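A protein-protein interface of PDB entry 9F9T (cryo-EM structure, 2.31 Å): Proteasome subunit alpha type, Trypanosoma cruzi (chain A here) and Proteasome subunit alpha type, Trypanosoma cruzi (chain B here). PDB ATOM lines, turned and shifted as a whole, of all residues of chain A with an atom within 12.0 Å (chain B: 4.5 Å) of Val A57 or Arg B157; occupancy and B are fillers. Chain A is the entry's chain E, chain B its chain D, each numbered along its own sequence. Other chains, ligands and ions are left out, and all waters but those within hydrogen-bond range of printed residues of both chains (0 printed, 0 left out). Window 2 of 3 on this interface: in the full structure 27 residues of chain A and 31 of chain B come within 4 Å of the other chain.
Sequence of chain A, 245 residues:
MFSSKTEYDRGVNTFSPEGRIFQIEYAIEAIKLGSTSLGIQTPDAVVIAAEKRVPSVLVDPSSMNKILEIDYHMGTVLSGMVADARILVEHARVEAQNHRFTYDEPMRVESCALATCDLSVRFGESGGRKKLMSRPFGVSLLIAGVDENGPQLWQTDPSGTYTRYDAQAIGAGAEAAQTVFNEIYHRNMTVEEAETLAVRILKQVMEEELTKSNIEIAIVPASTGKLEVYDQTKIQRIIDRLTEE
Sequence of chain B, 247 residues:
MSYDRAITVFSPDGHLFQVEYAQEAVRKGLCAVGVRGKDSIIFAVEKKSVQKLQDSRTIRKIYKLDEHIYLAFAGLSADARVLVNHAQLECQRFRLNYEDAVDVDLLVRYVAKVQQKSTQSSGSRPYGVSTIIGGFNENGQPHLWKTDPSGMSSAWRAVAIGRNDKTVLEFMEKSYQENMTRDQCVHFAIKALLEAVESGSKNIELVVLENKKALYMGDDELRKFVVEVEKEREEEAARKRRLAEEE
N of Arg B36 sits at hydrogen-bond distance from O of Arg B157 (3.1 Å). O of Arg B36 sits at hydrogen-bond distance from OH of Tyr B176 (2.5 Å). N of Trp B156 is in hydrogen-bond range of O of Leu B144 (2.9 Å). The side-chain carboxylate (OE2) of Glu B178 lies within salt-bridge range of the guanidinium group (NE) of Arg B157, at 3.7 Å. OG of Ser A63 lies within hydrogen-bond range of O of Asp A60 (3.1 Å).
The side-chain carboxylate (OD2) of Asp A60 is in salt-bridge range of the guanidinium group (NH1) of Arg B36 (3.3 Å). NH2 of Arg B157 lies within hydrogen-bond range of O of Val A57 (2.8 Å). The backbone NH (N) of Arg B157 sits at hydrogen-bond distance from the backbone carbonyl oxygen (O) of Leu A58 (2.7 Å). The backbone carbonyl oxygen (O) of Val A59 sits at hydrogen-bond distance from the guanidinium group (NH2) of Arg B157, at 3.1 Å. The guanidinium group (NE) of Arg B157 lies within salt-bridge range of the side-chain carboxylate (OD1) of Asp A60, at 3.1 Å.
Of the printed residues of chain B, Ser A56 touches Trp B156. Of chain B, only Arg B157 comes within 4 Å of Val A57. Of the printed residues of chain B, Leu A58 touches Trp B156 (3.4 Å), Arg B157 (2.7 Å), Ala B158 (3.6 Å) and Tyr B176 (3.8 Å). Printed residues of chain B within 4 Å of Val A59: Trp B156 (3.5 Å) and Arg B157 (3.1 Å). No residue of chain A comes within 4 Å of Val B35. Of chain A, only Ser A56 (3.2 Å), Leu A58 (3.4 Å) and Val A59 (3.5 Å) come within 4 Å of Trp B156. Of chain A, only Val A57, Leu A58, Val A59 and Asp A60 come within 4 Å of Arg B157. Of chain A, only Leu A58 comes within 4 Å of Ala B158. The nearest printed residue of chain B that does not touch Leu A58 is Arg B36 (6.6 Å).
Ser A56 touches Trp B156 (OG to CZ3, 3.2 Å). O of Leu A58 touches CA of Trp B156, 3.4 Å away. CB of Leu A58 touches O of Ala B158, 3.6 Å away. Tyr B176 touches Leu A58 (CB to CD2, 3.8 Å). Val A59 touches Trp B156 (CG2 to CZ2, 3.5 Å).
Of the 19 printed residues of chain A, 5 touch a printed residue of chain B. Printed residues of chain A that touch a printed residue of chain B: Ser A56, Val A57, Leu A58, Val A59 and Asp A60. Along chain A the printed residues that touch a printed residue of chain B span positions 56 to 60. Hydrophobic or aromatic side chains of chain B within 4 Å of the printed part of chain A: Trp B156 and Tyr B176. Along chain B the printed residues that touch a printed residue of chain A span positions 36 to 176.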
ATOM      1  N   LYS A  52     -23.275  21.830  11.982  1.00  0.00           N
ATOM      2  CA  LYS A  52     -22.553  21.336  13.146  1.00  0.00           C
ATOM      3  C   LYS A  52     -21.532  20.277  12.730  1.00  0.00           C
ATOM      4  O   LYS A  52     -20.332  20.474  12.916  1.00  0.00           O
ATOM      5  CB  LYS A  52     -23.505  20.851  14.242  1.00  0.00           C
ATOM      6  CG  LYS A  52     -23.815  21.924  15.275  1.00  0.00           C
ATOM      7  CD  LYS A  52     -24.243  21.410  16.623  1.00  0.00           C
ATOM      8  CE  LYS A  52     -24.163  22.486  17.687  1.00  0.00           C
ATOM      9  NZ  LYS A  52     -25.298  22.434  18.650  1.00  0.00           N
ATOM     10  N   ARG A  53     -22.014  19.158  12.188  1.00  0.00           N
ATOM     11  CA  ARG A  53     -21.159  18.073  11.726  1.00  0.00           C
ATOM     12  C   ARG A  53     -20.479  17.392  12.913  1.00  0.00           C
ATOM     13  O   ARG A  53     -19.267  17.491  13.083  1.00  0.00           O
ATOM     14  CB  ARG A  53     -20.136  18.543  10.683  1.00  0.00           C
ATOM     15  CG  ARG A  53     -19.573  17.408   9.833  1.00  0.00           C
ATOM     16  CD  ARG A  53     -18.296  17.753   9.074  1.00  0.00           C
ATOM     17  NE  ARG A  53     -18.511  18.357   7.761  1.00  0.00           N
ATOM     18  CZ  ARG A  53     -17.569  18.974   7.047  1.00  0.00           C
ATOM     19  NH1 ARG A  53     -17.850  19.462   5.849  1.00  0.00           N
ATOM     20  NH2 ARG A  53     -16.349  19.113   7.542  1.00  0.00           N
ATOM     21  N   VAL A  54     -21.289  16.648  13.679  1.00  0.00           N
ATOM     22  CA  VAL A  54     -20.817  15.702  14.686  1.00  0.00           C
ATOM     23  C   VAL A  54     -20.222  14.465  13.998  1.00  0.00           C
ATOM     24  O   VAL A  54     -20.709  14.033  12.946  1.00  0.00           O
ATOM     25  CB  VAL A  54     -21.946  15.287  15.663  1.00  0.00           C
ATOM     26  CG1 VAL A  54     -22.687  16.493  16.246  1.00  0.00           C
ATOM     27  CG2 VAL A  54     -22.923  14.299  15.025  1.00  0.00           C
ATOM     28  N   PRO A  55     -19.156  13.851  14.575  1.00  0.00           N
ATOM     29  CA  PRO A  55     -18.668  12.537  14.127  1.00  0.00           C
ATOM     30  C   PRO A  55     -19.303  11.280  14.743  1.00  0.00           C
ATOM     31  O   PRO A  55     -18.718  10.208  14.630  1.00  0.00           O
ATOM     32  CB  PRO A  55     -17.182  12.634  14.526  1.00  0.00           C
ATOM     33  CG  PRO A  55     -17.195  13.421  15.830  1.00  0.00           C
ATOM     34  CD  PRO A  55     -18.312  14.427  15.638  1.00  0.00           C
ATOM     35  N   SER A  56     -20.462  11.409  15.405  1.00  0.00           N
ATOM     36  CA  SER A  56     -21.337  10.287  15.709  1.00  0.00           C
ATOM     37  C   SER A  56     -22.492  10.712  16.613  1.00  0.00           C
ATOM     38  O   SER A  56     -22.542  11.852  17.060  1.00  0.00           O
ATOM     39  CB  SER A  56     -20.590   9.113  16.325  1.00  0.00           C
ATOM     40  OG  SER A  56     -19.791   9.500  17.428  1.00  0.00           O
ATOM     41  N   VAL A  57     -23.376   9.758  16.923  1.00  0.00           N
ATOM     42  CA  VAL A  57     -24.593  10.006  17.680  1.00  0.00           C
ATOM     43  C   VAL A  57     -24.357   9.756  19.172  1.00  0.00           C
ATOM     44  O   VAL A  57     -25.308   9.799  19.963  1.00  0.00           O
ATOM     45  CB  VAL A  57     -25.760   9.146  17.140  1.00  0.00           C
ATOM     46  CG1 VAL A  57     -25.773   9.135  15.619  1.00  0.00           C
ATOM     47  CG2 VAL A  57     -25.751   7.713  17.680  1.00  0.00           C
ATOM     48  N   LEU A  58     -23.090   9.473  19.533  1.00  0.00           N
ATOM     49  CA  LEU A  58     -22.650   9.381  20.927  1.00  0.00           C
ATOM     50  C   LEU A  58     -22.111  10.717  21.440  1.00  0.00           C
ATOM     51  O   LEU A  58     -22.077  10.908  22.650  1.00  0.00           O
ATOM     52  CB  LEU A  58     -21.588   8.286  21.056  1.00  0.00           C
ATOM     53  CG  LEU A  58     -22.069   6.880  20.688  1.00  0.00           C
ATOM     54  CD1 LEU A  58     -20.918   5.892  20.707  1.00  0.00           C
ATOM     55  CD2 LEU A  58     -23.190   6.420  21.607  1.00  0.00           C
ATOM     56  N   VAL A  59     -21.759  11.644  20.528  1.00  0.00           N
ATOM     57  CA  VAL A  59     -21.419  13.012  20.907  1.00  0.00           C
ATOM     58  C   VAL A  59     -22.639  13.762  21.434  1.00  0.00           C
ATOM     59  O   VAL A  59     -23.670  13.736  20.781  1.00  0.00           O
ATOM     60  CB  VAL A  59     -20.820  13.786  19.729  1.00  0.00           C
ATOM     61  CG1 VAL A  59     -20.600  15.249  20.088  1.00  0.00           C
ATOM     62  CG2 VAL A  59     -19.526  13.155  19.240  1.00  0.00           C
ATOM     63  N   ASP A  60     -22.510  14.440  22.594  1.00  0.00           N
ATOM     64  CA  ASP A  60     -23.489  15.431  23.055  1.00  0.00           C
ATOM     65  C   ASP A  60     -23.347  16.692  22.202  1.00  0.00           C
ATOM     66  O   ASP A  60     -22.266  17.274  22.164  1.00  0.00           O
ATOM     67  CB  ASP A  60     -23.312  15.863  24.519  1.00  0.00           C
ATOM     68  CG  ASP A  60     -23.946  14.980  25.582  1.00  0.00           C
ATOM     69  OD1 ASP A  60     -24.410  13.869  25.243  1.00  0.00           O
ATOM     70  OD2 ASP A  60     -24.004  15.429  26.749  1.00  0.00           O
ATOM     71  N   PRO A  61     -24.384  17.156  21.463  1.00  0.00           N
ATOM     72  CA  PRO A  61     -24.160  18.135  20.392  1.00  0.00           C
ATOM     73  C   PRO A  61     -23.904  19.560  20.905  1.00  0.00           C
ATOM     74  O   PRO A  61     -23.157  20.304  20.267  1.00  0.00           O
ATOM     75  CB  PRO A  61     -25.423  17.997  19.516  1.00  0.00           C
ATOM     76  CG  PRO A  61     -26.196  16.811  20.107  1.00  0.00           C
ATOM     77  CD  PRO A  61     -25.797  16.758  21.570  1.00  0.00           C
ATOM     78  N   SER A  62     -24.477  19.903  22.080  1.00  0.00           N
ATOM     79  CA  SER A  62     -24.179  21.131  22.824  1.00  0.00           C
ATOM     80  C   SER A  62     -22.706  21.549  22.691  1.00  0.00           C
ATOM     81  O   SER A  62     -22.398  22.687  22.359  1.00  0.00           O
ATOM     82  CB  SER A  62     -24.548  20.977  24.292  1.00  0.00           C
ATOM     83  OG  SER A  62     -25.438  19.885  24.489  1.00  0.00           O
ATOM     84  N   SER A  63     -21.796  20.599  22.919  1.00  0.00           N
ATOM     85  CA  SER A  63     -20.391  20.840  23.201  1.00  0.00           C
ATOM     86  C   SER A  63     -19.582  21.234  21.964  1.00  0.00           C
ATOM     87  O   SER A  63     -18.422  21.631  22.091  1.00  0.00           O
ATOM     88  CB  SER A  63     -19.815  19.591  23.808  1.00  0.00           C
ATOM     89  OG  SER A  63     -19.518  18.632  22.806  1.00  0.00           O
ATOM     90  N   MET A  64     -20.205  21.127  20.781  1.00  0.00           N
ATOM     91  CA  MET A  64     -19.540  21.324  19.503  1.00  0.00           C
ATOM     92  C   MET A  64     -20.028  22.603  18.810  1.00  0.00           C
ATOM     93  O   MET A  64     -20.266  22.607  17.602  1.00  0.00           O
ATOM     94  CB  MET A  64     -19.845  20.113  18.619  1.00  0.00           C
ATOM     95  CG  MET A  64     -19.256  18.827  19.163  1.00  0.00           C
ATOM     96  SD  MET A  64     -18.632  17.759  17.847  1.00  0.00           S
ATOM     97  CE  MET A  64     -16.924  18.289  17.746  1.00  0.00           C
ATOM     98  N   GLU A 208     -25.521  15.605   4.864  1.00  0.00           N
ATOM     99  CA  GLU A 208     -26.535  14.922   5.656  1.00  0.00           C
ATOM    100  C   GLU A 208     -27.927  15.411   5.254  1.00  0.00           C
ATOM    101  O   GLU A 208     -28.068  16.354   4.476  1.00  0.00           O
ATOM    102  CB  GLU A 208     -26.297  15.176   7.151  1.00  0.00           C
ATOM    103  CG  GLU A 208     -24.987  14.606   7.693  1.00  0.00           C
ATOM    104  CD  GLU A 208     -24.514  15.163   9.033  1.00  0.00           C
ATOM    105  OE1 GLU A 208     -24.027  16.316   9.062  1.00  0.00           O
ATOM    106  OE2 GLU A 208     -24.627  14.441  10.049  1.00  0.00           O
ATOM    107  N   GLU A 209     -28.952  14.735   5.789  1.00  0.00           N
ATOM    108  CA  GLU A 209     -30.284  15.305   5.888  1.00  0.00           C
ATOM    109  C   GLU A 209     -30.265  16.336   7.011  1.00  0.00           C
ATOM    110  O   GLU A 209     -29.540  16.172   7.993  1.00  0.00           O
ATOM    111  CB  GLU A 209     -31.347  14.238   6.175  1.00  0.00           C
ATOM    112  CG  GLU A 209     -31.573  13.263   5.028  1.00  0.00           C
ATOM    113  CD  GLU A 209     -32.753  12.316   5.191  1.00  0.00           C
ATOM    114  OE1 GLU A 209     -33.502  12.460   6.181  1.00  0.00           O
ATOM    115  OE2 GLU A 209     -32.921  11.431   4.327  1.00  0.00           O
ATOM    116  N   THR A 211     -31.666  18.728  10.052  1.00  0.00           N
ATOM    117  CA  THR A 211     -32.466  18.527  11.247  1.00  0.00           C
ATOM    118  C   THR A 211     -32.192  19.673  12.216  1.00  0.00           C
ATOM    119  O   THR A 211     -31.203  20.387  12.067  1.00  0.00           O
ATOM    120  CB  THR A 211     -32.166  17.171  11.909  1.00  0.00           C
ATOM    121  OG1 THR A 211     -30.984  17.274  12.703  1.00  0.00           O
ATOM    122  CG2 THR A 211     -31.999  16.037  10.919  1.00  0.00           C
ATOM    123  N   SER A 213     -31.240  19.594  15.248  1.00  0.00           N
ATOM    124  CA  SER A 213     -30.080  19.363  16.100  1.00  0.00           C
ATOM    125  C   SER A 213     -28.780  19.623  15.340  1.00  0.00           C
ATOM    126  O   SER A 213     -27.739  19.865  15.947  1.00  0.00           O
ATOM    127  CB  SER A 213     -30.111  17.958  16.658  1.00  0.00           C
ATOM    128  OG  SER A 213     -30.231  16.992  15.620  1.00  0.00           O
ATOM    129  N   ASN A 214     -28.883  19.620  14.006  1.00  0.00           N
ATOM    130  CA  ASN A 214     -27.760  19.523  13.086  1.00  0.00           C
ATOM    131  C   ASN A 214     -27.258  20.913  12.645  1.00  0.00           C
ATOM    132  O   ASN A 214     -26.257  21.020  11.925  1.00  0.00           O
ATOM    133  CB  ASN A 214     -28.205  18.679  11.884  1.00  0.00           C
ATOM    134  CG  ASN A 214     -27.071  18.071  11.089  1.00  0.00           C
ATOM    135  OD1 ASN A 214     -26.000  17.790  11.623  1.00  0.00           O
ATOM    136  ND2 ASN A 214     -27.315  17.831   9.812  1.00  0.00           N
ATOM    137  N   GLN A 232     -33.920  24.704  19.693  1.00  0.00           N
ATOM    138  CA  GLN A 232     -34.274  23.735  18.661  1.00  0.00           C
ATOM    139  C   GLN A 232     -35.773  23.826  18.346  1.00  0.00           C
ATOM    140  O   GLN A 232     -36.207  23.436  17.261  1.00  0.00           O
ATOM    141  CB  GLN A 232     -33.871  22.323  19.099  1.00  0.00           C
ATOM    142  CG  GLN A 232     -32.383  22.046  18.959  1.00  0.00           C
ATOM    143  CD  GLN A 232     -31.982  20.784  19.680  1.00  0.00           C
ATOM    144  OE1 GLN A 232     -32.273  20.595  20.861  1.00  0.00           O
ATOM    145  NE2 GLN A 232     -31.313  19.899  18.962  1.00  0.00           N
ATOM    146  N   VAL B  35     -17.602   5.399  29.413  1.00  0.00           N
ATOM    147  CA  VAL B  35     -19.017   5.145  29.283  1.00  0.00           C
ATOM    148  C   VAL B  35     -19.726   5.838  30.422  1.00  0.00           C
ATOM    149  O   VAL B  35     -19.509   5.526  31.588  1.00  0.00           O
ATOM    150  CB  VAL B  35     -19.370   3.645  29.346  1.00  0.00           C
ATOM    151  CG1 VAL B  35     -20.867   3.409  29.086  1.00  0.00           C
ATOM    152  CG2 VAL B  35     -18.522   2.778  28.412  1.00  0.00           C
ATOM    153  N   ARG B  36     -20.656   6.697  30.058  1.00  0.00           N
ATOM    154  CA  ARG B  36     -21.347   7.517  31.023  1.00  0.00           C
ATOM    155  C   ARG B  36     -22.697   6.876  31.334  1.00  0.00           C
ATOM    156  O   ARG B  36     -23.540   6.744  30.454  1.00  0.00           O
ATOM    157  CB  ARG B  36     -21.456   8.903  30.396  1.00  0.00           C
ATOM    158  CG  ARG B  36     -21.777  10.031  31.351  1.00  0.00           C
ATOM    159  CD  ARG B  36     -22.245  11.240  30.587  1.00  0.00           C
ATOM    160  NE  ARG B  36     -23.641  11.118  30.194  1.00  0.00           N
ATOM    161  CZ  ARG B  36     -24.236  11.931  29.340  1.00  0.00           C
ATOM    162  NH1 ARG B  36     -23.548  12.897  28.770  1.00  0.00           N
ATOM    163  NH2 ARG B  36     -25.506  11.767  29.024  1.00  0.00           N
ATOM    164  N   LEU B 144     -18.372  13.390  30.319  1.00  0.00           N
ATOM    165  CA  LEU B 144     -17.279  12.647  29.730  1.00  0.00           C
ATOM    166  C   LEU B 144     -16.747  13.388  28.520  1.00  0.00           C
ATOM    167  O   LEU B 144     -17.497  13.680  27.609  1.00  0.00           O
ATOM    168  CB  LEU B 144     -17.750  11.225  29.407  1.00  0.00           C
ATOM    169  CG  LEU B 144     -16.825  10.361  28.546  1.00  0.00           C
ATOM    170  CD1 LEU B 144     -15.569   9.973  29.277  1.00  0.00           C
ATOM    171  CD2 LEU B 144     -17.521   9.077  28.145  1.00  0.00           C
ATOM    172  N   TRP B 156     -19.107  13.361  25.247  1.00  0.00           N
ATOM    173  CA  TRP B 156     -19.666  12.122  24.720  1.00  0.00           C
ATOM    174  C   TRP B 156     -20.467  11.365  25.740  1.00  0.00           C
ATOM    175  O   TRP B 156     -20.263  11.515  26.937  1.00  0.00           O
ATOM    176  CB  TRP B 156     -18.558  11.192  24.272  1.00  0.00           C
ATOM    177  CG  TRP B 156     -17.746  11.757  23.156  1.00  0.00           C
ATOM    178  CD1 TRP B 156     -16.861  12.781  23.240  1.00  0.00           C
ATOM    179  CD2 TRP B 156     -17.609  11.237  21.827  1.00  0.00           C
ATOM    180  NE1 TRP B 156     -16.221  12.988  22.044  1.00  0.00           N
ATOM    181  CE2 TRP B 156     -16.667  12.057  21.155  1.00  0.00           C
ATOM    182  CE3 TRP B 156     -18.176  10.160  21.151  1.00  0.00           C
ATOM    183  CZ2 TRP B 156     -16.296  11.846  19.839  1.00  0.00           C
ATOM    184  CZ3 TRP B 156     -17.804   9.950  19.848  1.00  0.00           C
ATOM    185  CH2 TRP B 156     -16.863  10.764  19.210  1.00  0.00           C
ATOM    186  N   ARG B 157     -21.334  10.495  25.237  1.00  0.00           N
ATOM    187  CA  ARG B 157     -22.051   9.543  26.066  1.00  0.00           C
ATOM    188  C   ARG B 157     -21.269   8.227  26.151  1.00  0.00           C
ATOM    189  O   ARG B 157     -21.310   7.516  27.144  1.00  0.00           O
ATOM    190  CB  ARG B 157     -23.465   9.436  25.496  1.00  0.00           C
ATOM    191  CG  ARG B 157     -24.404  10.463  26.130  1.00  0.00           C
ATOM    192  CD  ARG B 157     -25.818  10.457  25.576  1.00  0.00           C
ATOM    193  NE  ARG B 157     -25.829  11.254  24.363  1.00  0.00           N
ATOM    194  CZ  ARG B 157     -25.695  10.775  23.133  1.00  0.00           C
ATOM    195  NH1 ARG B 157     -25.869   9.485  22.888  1.00  0.00           N
ATOM    196  NH2 ARG B 157     -25.434  11.616  22.144  1.00  0.00           N
ATOM    197  N   ALA B 158     -20.500   7.922  25.117  1.00  0.00           N
ATOM    198  CA  ALA B 158     -19.455   6.951  25.295  1.00  0.00           C
ATOM    199  C   ALA B 158     -18.427   7.120  24.191  1.00  0.00           C
ATOM    200  O   ALA B 158     -18.750   7.689  23.159  1.00  0.00           O
ATOM    201  CB  ALA B 158     -20.077   5.587  25.320  1.00  0.00           C
ATOM    202  N   TYR B 176     -25.558   1.332  22.780  1.00  0.00           N
ATOM    203  CA  TYR B 176     -25.509   2.263  23.905  1.00  0.00           C
ATOM    204  C   TYR B 176     -26.944   2.538  24.380  1.00  0.00           C
ATOM    205  O   TYR B 176     -27.887   2.525  23.591  1.00  0.00           O
ATOM    206  CB  TYR B 176     -24.710   3.546  23.584  1.00  0.00           C
ATOM    207  CG  TYR B 176     -24.687   4.511  24.771  1.00  0.00           C
ATOM    208  CD1 TYR B 176     -23.812   4.304  25.835  1.00  0.00           C
ATOM    209  CD2 TYR B 176     -25.618   5.541  24.904  1.00  0.00           C
ATOM    210  CE1 TYR B 176     -23.825   5.107  26.967  1.00  0.00           C
ATOM    211  CE2 TYR B 176     -25.647   6.347  26.037  1.00  0.00           C
ATOM    212  CZ  TYR B 176     -24.734   6.144  27.070  1.00  0.00           C
ATOM    213  OH  TYR B 176     -24.692   6.937  28.191  1.00  0.00           O
ATOM    214  N   GLU B 178     -29.382   4.890  27.361  1.00  0.00           N
ATOM    215  CA  GLU B 178     -29.448   5.973  28.324  1.00  0.00           C
ATOM    216  C   GLU B 178     -29.737   5.368  29.699  1.00  0.00           C
ATOM    217  O   GLU B 178     -30.456   4.369  29.796  1.00  0.00           O
ATOM    218  CB  GLU B 178     -30.496   7.008  27.882  1.00  0.00           C
ATOM    219  CG  GLU B 178     -29.946   8.241  27.148  1.00  0.00           C
ATOM    220  CD  GLU B 178     -29.055   8.060  25.921  1.00  0.00           C
ATOM    221  OE1 GLU B 178     -28.761   6.901  25.544  1.00  0.00           O
ATOM    222  OE2 GLU B 178     -28.650   9.092  25.334  1.00  0.00           O
